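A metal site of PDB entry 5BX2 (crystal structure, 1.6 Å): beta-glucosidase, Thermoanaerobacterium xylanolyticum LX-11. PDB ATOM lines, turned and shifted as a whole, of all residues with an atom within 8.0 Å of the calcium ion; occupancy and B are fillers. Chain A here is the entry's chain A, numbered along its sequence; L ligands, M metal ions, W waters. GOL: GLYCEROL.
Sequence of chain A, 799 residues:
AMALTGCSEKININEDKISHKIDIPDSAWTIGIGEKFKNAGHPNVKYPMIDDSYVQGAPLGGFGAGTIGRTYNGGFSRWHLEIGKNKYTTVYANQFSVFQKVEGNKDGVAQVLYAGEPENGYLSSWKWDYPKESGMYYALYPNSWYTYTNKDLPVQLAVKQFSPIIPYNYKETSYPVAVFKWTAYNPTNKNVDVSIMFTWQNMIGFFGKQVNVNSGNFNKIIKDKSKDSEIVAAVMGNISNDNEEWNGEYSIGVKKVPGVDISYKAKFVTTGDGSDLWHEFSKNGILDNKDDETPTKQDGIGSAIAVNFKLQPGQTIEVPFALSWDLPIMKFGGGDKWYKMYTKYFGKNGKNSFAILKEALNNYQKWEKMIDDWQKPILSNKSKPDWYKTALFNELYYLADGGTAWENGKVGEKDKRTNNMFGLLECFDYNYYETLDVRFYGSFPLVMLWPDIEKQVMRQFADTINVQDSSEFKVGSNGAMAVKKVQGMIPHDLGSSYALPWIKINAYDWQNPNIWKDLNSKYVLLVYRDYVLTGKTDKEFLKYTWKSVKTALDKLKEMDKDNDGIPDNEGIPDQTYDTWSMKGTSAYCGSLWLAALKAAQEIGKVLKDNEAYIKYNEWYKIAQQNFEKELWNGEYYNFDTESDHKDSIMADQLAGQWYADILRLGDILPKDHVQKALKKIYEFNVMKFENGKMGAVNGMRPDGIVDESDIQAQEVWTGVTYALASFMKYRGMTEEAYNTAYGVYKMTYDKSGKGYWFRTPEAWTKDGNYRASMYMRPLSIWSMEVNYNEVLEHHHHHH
OD2 of Asp 564 sits close to OE2 of Glu 630, 2.6 Å away. OD2 of Asp 560 lies close to N of Asn 563 (3.5 Å). OD1 of Asp 568 sits close to N of Lys 561, 2.9 Å away. OD2 of Asp 564 sits at hydrogen-bond distance from OG1 of Thr 585, 3.0 Å away. The side-chain carboxylate (OD2) of Asp 560 sits at hydrogen-bond distance from the backbone NH (N) of Gly 565, 2.8 Å away. O of Asp 564 sits at hydrogen-bond distance from ND2 of Asn 626, 2.9 Å away. The backbone NH (N) of Asp 568 lies within hydrogen-bond range of the backbone carbonyl oxygen (O) of Met 559, 3.0 Å away.
The nearest printed residue that does not touch the calcium ion is Lys 561 (4.2 Å).
OD1 of Asp 568 is bound to the calcium ion, 2.2 Å away. Water W1 is bound to the calcium ion. The side-chain carboxylate (OD1) of Asp 564 binds the calcium ion (2.4 Å). The calcium ion is bound by the backbone carbonyl oxygen (O) of Ile 566 (2.4 Å). The calcium ion is bound by the side-chain carboxylate (OD1) of Asp 562 (2.4 Å). The calcium ion is bound by OD1 of Asp 560. O3 of the ligand is bound to the calcium ion (2.6 Å). The calcium ion has seven donor atoms within binding distance.
Water W1 bridges OG1 of Thr 585 (2.6 Å) and O of Pro 567 (3.0 Å).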
ATOM      1  N   LYS A 557     -25.413 -11.930  28.159  1.00  0.00           N
ATOM      2  CA  LYS A 557     -24.371 -11.315  27.325  1.00  0.00           C
ATOM      3  C   LYS A 557     -24.244 -12.022  25.983  1.00  0.00           C
ATOM      4  O   LYS A 557     -23.950 -11.379  24.982  1.00  0.00           O
ATOM      5  CB  LYS A 557     -23.025 -11.331  28.064  1.00  0.00           C
ATOM      6  CG  LYS A 557     -21.872 -10.639  27.340  1.00  0.00           C
ATOM      7  CD  LYS A 557     -22.236  -9.225  26.902  1.00  0.00           C
ATOM      8  CE  LYS A 557     -21.043  -8.294  26.912  1.00  0.00           C
ATOM      9  NZ  LYS A 557     -19.900  -8.803  26.110  1.00  0.00           N
ATOM     10  N   MET A 559     -26.549 -13.048  24.161  1.00  0.00           N
ATOM     11  CA  MET A 559     -27.621 -12.608  23.273  1.00  0.00           C
ATOM     12  C   MET A 559     -27.340 -11.259  22.598  1.00  0.00           C
ATOM     13  O   MET A 559     -28.178 -10.719  21.905  1.00  0.00           O
ATOM     14  CB  MET A 559     -28.942 -12.569  24.027  1.00  0.00           C
ATOM     15  CG  MET A 559     -29.426 -13.957  24.442  1.00  0.00           C
ATOM     16  SD  MET A 559     -30.800 -13.855  25.596  1.00  0.00           S
ATOM     17  CE  MET A 559     -31.135 -15.603  25.807  1.00  0.00           C
ATOM     18  N   ASP A 560     -26.140 -10.718  22.812  1.00  0.00           N
ATOM     19  CA  ASP A 560     -25.683  -9.550  22.062  1.00  0.00           C
ATOM     20  C   ASP A 560     -25.213 -10.030  20.692  1.00  0.00           C
ATOM     21  O   ASP A 560     -24.171 -10.666  20.581  1.00  0.00           O
ATOM     22  CB  ASP A 560     -24.555  -8.859  22.824  1.00  0.00           C
ATOM     23  CG  ASP A 560     -23.966  -7.678  22.071  1.00  0.00           C
ATOM     24  OD1 ASP A 560     -24.590  -7.131  21.138  1.00  0.00           O
ATOM     25  OD2 ASP A 560     -22.840  -7.288  22.454  1.00  0.00           O
ATOM     26  N   LYS A 561     -25.985  -9.730  19.650  1.00  0.00           N
ATOM     27  CA  LYS A 561     -25.696 -10.221  18.293  1.00  0.00           C
ATOM     28  C   LYS A 561     -24.593  -9.428  17.601  1.00  0.00           C
ATOM     29  O   LYS A 561     -23.829  -9.988  16.812  1.00  0.00           O
ATOM     30  CB  LYS A 561     -26.959 -10.145  17.425  1.00  0.00           C
ATOM     31  CG  LYS A 561     -28.055 -11.125  17.824  1.00  0.00           C
ATOM     32  CD  LYS A 561     -29.342 -10.837  17.050  1.00  0.00           C
ATOM     33  CE  LYS A 561     -30.353 -11.952  17.234  1.00  0.00           C
ATOM     34  NZ  LYS A 561     -31.664 -11.618  16.601  1.00  0.00           N
ATOM     35  N   ASP A 562     -24.497  -8.137  17.900  1.00  0.00           N
ATOM     36  CA  ASP A 562     -23.653  -7.204  17.124  1.00  0.00           C
ATOM     37  C   ASP A 562     -22.523  -6.561  17.917  1.00  0.00           C
ATOM     38  O   ASP A 562     -21.976  -5.541  17.512  1.00  0.00           O
ATOM     39  CB  ASP A 562     -24.543  -6.120  16.510  1.00  0.00           C
ATOM     40  CG  ASP A 562     -25.157  -5.214  17.555  1.00  0.00           C
ATOM     41  OD1 ASP A 562     -25.248  -5.615  18.747  1.00  0.00           O
ATOM     42  OD2 ASP A 562     -25.569  -4.093  17.198  1.00  0.00           O
ATOM     43  N   ASN A 563     -22.186  -7.155  19.054  1.00  0.00           N
ATOM     44  CA  ASN A 563     -21.077  -6.679  19.887  1.00  0.00           C
ATOM     45  C   ASN A 563     -21.110  -5.180  20.258  1.00  0.00           C
ATOM     46  O   ASN A 563     -20.060  -4.538  20.337  1.00  0.00           O
ATOM     47  CB  ASN A 563     -19.732  -7.052  19.242  1.00  0.00           C
ATOM     48  CG  ASN A 563     -18.571  -6.989  20.224  1.00  0.00           C
ATOM     49  OD1 ASN A 563     -18.743  -7.144  21.435  1.00  0.00           O
ATOM     50  ND2 ASN A 563     -17.372  -6.745  19.704  1.00  0.00           N
ATOM     51  N   ASP A 564     -22.302  -4.634  20.504  1.00  0.00           N
ATOM     52  CA  ASP A 564     -22.395  -3.301  21.111  1.00  0.00           C
ATOM     53  C   ASP A 564     -22.446  -3.411  22.653  1.00  0.00           C
ATOM     54  O   ASP A 564     -22.549  -2.403  23.357  1.00  0.00           O
ATOM     55  CB  ASP A 564     -23.601  -2.504  20.570  1.00  0.00           C
ATOM     56  CG  ASP A 564     -24.935  -2.943  21.158  1.00  0.00           C
ATOM     57  OD1 ASP A 564     -25.004  -4.054  21.707  1.00  0.00           O
ATOM     58  OD2 ASP A 564     -25.919  -2.177  21.055  1.00  0.00           O
ATOM     59  N   GLY A 565     -22.362  -4.633  23.168  1.00  0.00           N
ATOM     60  CA  GLY A 565     -22.297  -4.893  24.610  1.00  0.00           C
ATOM     61  C   GLY A 565     -23.650  -5.014  25.283  1.00  0.00           C
ATOM     62  O   GLY A 565     -23.725  -5.121  26.506  1.00  0.00           O
ATOM     63  N   ILE A 566     -24.716  -5.028  24.481  1.00  0.00           N
ATOM     64  CA  ILE A 566     -26.090  -5.049  24.992  1.00  0.00           C
ATOM     65  C   ILE A 566     -26.867  -6.180  24.311  1.00  0.00           C
ATOM     66  O   ILE A 566     -26.809  -6.323  23.088  1.00  0.00           O
ATOM     67  CB  ILE A 566     -26.799  -3.712  24.690  1.00  0.00           C
ATOM     68  CG1 ILE A 566     -25.959  -2.529  25.181  1.00  0.00           C
ATOM     69  CG2 ILE A 566     -28.182  -3.653  25.335  1.00  0.00           C
ATOM     70  CD1 ILE A 566     -26.479  -1.189  24.728  1.00  0.00           C
ATOM     71  N   PRO A 567     -27.606  -6.988  25.084  1.00  0.00           N
ATOM     72  CA  PRO A 567     -28.424  -8.025  24.422  1.00  0.00           C
ATOM     73  C   PRO A 567     -29.377  -7.426  23.400  1.00  0.00           C
ATOM     74  O   PRO A 567     -29.875  -6.325  23.598  1.00  0.00           O
ATOM     75  CB  PRO A 567     -29.191  -8.680  25.579  1.00  0.00           C
ATOM     76  CG  PRO A 567     -29.088  -7.736  26.718  1.00  0.00           C
ATOM     77  CD  PRO A 567     -27.813  -6.968  26.539  1.00  0.00           C
ATOM     78  N   ASP A 568     -29.615  -8.146  22.306  1.00  0.00           N
ATOM     79  CA  ASP A 568     -30.485  -7.701  21.223  1.00  0.00           C
ATOM     80  C   ASP A 568     -31.892  -8.265  21.400  1.00  0.00           C
ATOM     81  O   ASP A 568     -32.070  -9.478  21.344  1.00  0.00           O
ATOM     82  CB  ASP A 568     -29.972  -8.189  19.863  1.00  0.00           C
ATOM     83  CG  ASP A 568     -28.735  -7.435  19.386  1.00  0.00           C
ATOM     84  OD1 ASP A 568     -27.716  -7.406  20.107  1.00  0.00           O
ATOM     85  OD2 ASP A 568     -28.767  -6.895  18.249  1.00  0.00           O
ATOM     86  N   ASN A 569     -32.886  -7.399  21.562  1.00  0.00           N
ATOM     87  CA  ASN A 569     -34.278  -7.848  21.439  1.00  0.00           C
ATOM     88  C   ASN A 569     -34.489  -8.360  20.010  1.00  0.00           C
ATOM     89  O   ASN A 569     -33.925  -7.827  19.066  1.00  0.00           O
ATOM     90  CB  ASN A 569     -35.257  -6.724  21.781  1.00  0.00           C
ATOM     91  CG  ASN A 569     -35.223  -6.345  23.257  1.00  0.00           C
ATOM     92  OD1 ASN A 569     -34.587  -5.364  23.650  1.00  0.00           O
ATOM     93  ND2 ASN A 569     -35.929  -7.110  24.084  1.00  0.00           N
ATOM     94  N   GLY A 584     -33.480  -4.953  18.561  1.00  0.00           N
ATOM     95  CA  GLY A 584     -32.203  -4.281  18.736  1.00  0.00           C
ATOM     96  C   GLY A 584     -31.973  -3.930  20.199  1.00  0.00           C
ATOM     97  O   GLY A 584     -32.297  -4.723  21.079  1.00  0.00           O
ATOM     98  N   THR A 585     -31.410  -2.755  20.441  1.00  0.00           N
ATOM     99  CA  THR A 585     -31.268  -2.256  21.808  1.00  0.00           C
ATOM    100  C   THR A 585     -32.553  -1.542  22.182  1.00  0.00           C
ATOM    101  O   THR A 585     -32.973  -0.620  21.490  1.00  0.00           O
ATOM    102  CB  THR A 585     -30.067  -1.320  21.931  1.00  0.00           C
ATOM    103  OG1 THR A 585     -28.858  -2.074  21.740  1.00  0.00           O
ATOM    104  CG2 THR A 585     -30.043  -0.646  23.298  1.00  0.00           C
ATOM    105  N   ASN A 626     -22.757   2.929  24.646  1.00  0.00           N
ATOM    106  CA  ASN A 626     -23.546   2.608  23.470  1.00  0.00           C
ATOM    107  C   ASN A 626     -25.060   2.784  23.625  1.00  0.00           C
ATOM    108  O   ASN A 626     -25.742   3.143  22.673  1.00  0.00           O
ATOM    109  CB  ASN A 626     -23.218   1.199  22.977  1.00  0.00           C
ATOM    110  CG  ASN A 626     -21.835   1.111  22.366  1.00  0.00           C
ATOM    111  OD1 ASN A 626     -21.337   2.097  21.828  1.00  0.00           O
ATOM    112  ND2 ASN A 626     -21.200  -0.053  22.439  1.00  0.00           N
ATOM    113  N   GLU A 630     -27.040   5.175  21.098  1.00  0.00           N
ATOM    114  CA  GLU A 630     -28.062   4.593  20.266  1.00  0.00           C
ATOM    115  C   GLU A 630     -29.458   5.158  20.525  1.00  0.00           C
ATOM    116  O   GLU A 630     -30.273   5.250  19.602  1.00  0.00           O
ATOM    117  CB  GLU A 630     -28.105   3.085  20.461  1.00  0.00           C
ATOM    118  CG  GLU A 630     -26.870   2.347  19.955  1.00  0.00           C
ATOM    119  CD  GLU A 630     -26.757   0.937  20.486  1.00  0.00           C
ATOM    120  OE1 GLU A 630     -27.758   0.433  21.054  1.00  0.00           O
ATOM    121  OE2 GLU A 630     -25.681   0.331  20.354  1.00  0.00           O
ATOM    122  N   THR A 641     -33.917   0.497  18.838  1.00  0.00           N
ATOM    123  CA  THR A 641     -33.106   0.918  17.683  1.00  0.00           C
ATOM    124  C   THR A 641     -33.610   0.407  16.345  1.00  0.00           C
ATOM    125  O   THR A 641     -33.203   0.944  15.318  1.00  0.00           O
ATOM    126  CB  THR A 641     -31.637   0.496  17.848  1.00  0.00           C
ATOM    127  OG1 THR A 641     -31.568  -0.914  18.064  1.00  0.00           O
ATOM    128  CG2 THR A 641     -30.998   1.226  19.020  1.00  0.00           C
ATOM    129  N   GLU A 642     -34.476  -0.603  16.325  1.00  0.00           N
ATOM    130  CA  GLU A 642     -34.842  -1.274  15.060  1.00  0.00           C
ATOM    131  C   GLU A 642     -36.338  -1.453  14.725  1.00  0.00           C
ATOM    132  O   GLU A 642     -36.672  -1.768  13.584  1.00  0.00           O
ATOM    133  CB  GLU A 642     -34.134  -2.632  14.981  1.00  0.00           C
ATOM    134  CG  GLU A 642     -32.610  -2.535  14.989  1.00  0.00           C
ATOM    135  CD  GLU A 642     -31.913  -3.869  14.803  1.00  0.00           C
ATOM    136  OE1 GLU A 642     -32.434  -4.720  14.051  1.00  0.00           O
ATOM    137  OE2 GLU A 642     -30.834  -4.070  15.388  1.00  0.00           O
HETATM  138  C1  GOL L   1     -27.859  -1.174  18.170  1.00  0.00           C
HETATM  139  O1  GOL L   1     -27.736  -0.091  17.249  1.00  0.00           O
HETATM  140  C2  GOL L   1     -28.402  -2.407  17.452  1.00  0.00           C
HETATM  141  O2  GOL L   1     -29.643  -2.066  16.816  1.00  0.00           O
HETATM  142  C3  GOL L   1     -28.649  -3.549  18.437  1.00  0.00           C
HETATM  143  O3  GOL L   1     -27.432  -4.125  18.921  1.00  0.00           O
HETATM  144 CA    CA M   1     -26.496  -5.679  20.810  1.00  0.00          CA
HETATM  145  O   HOH W   1     -28.543  -4.665  21.467  1.00  0.00           O
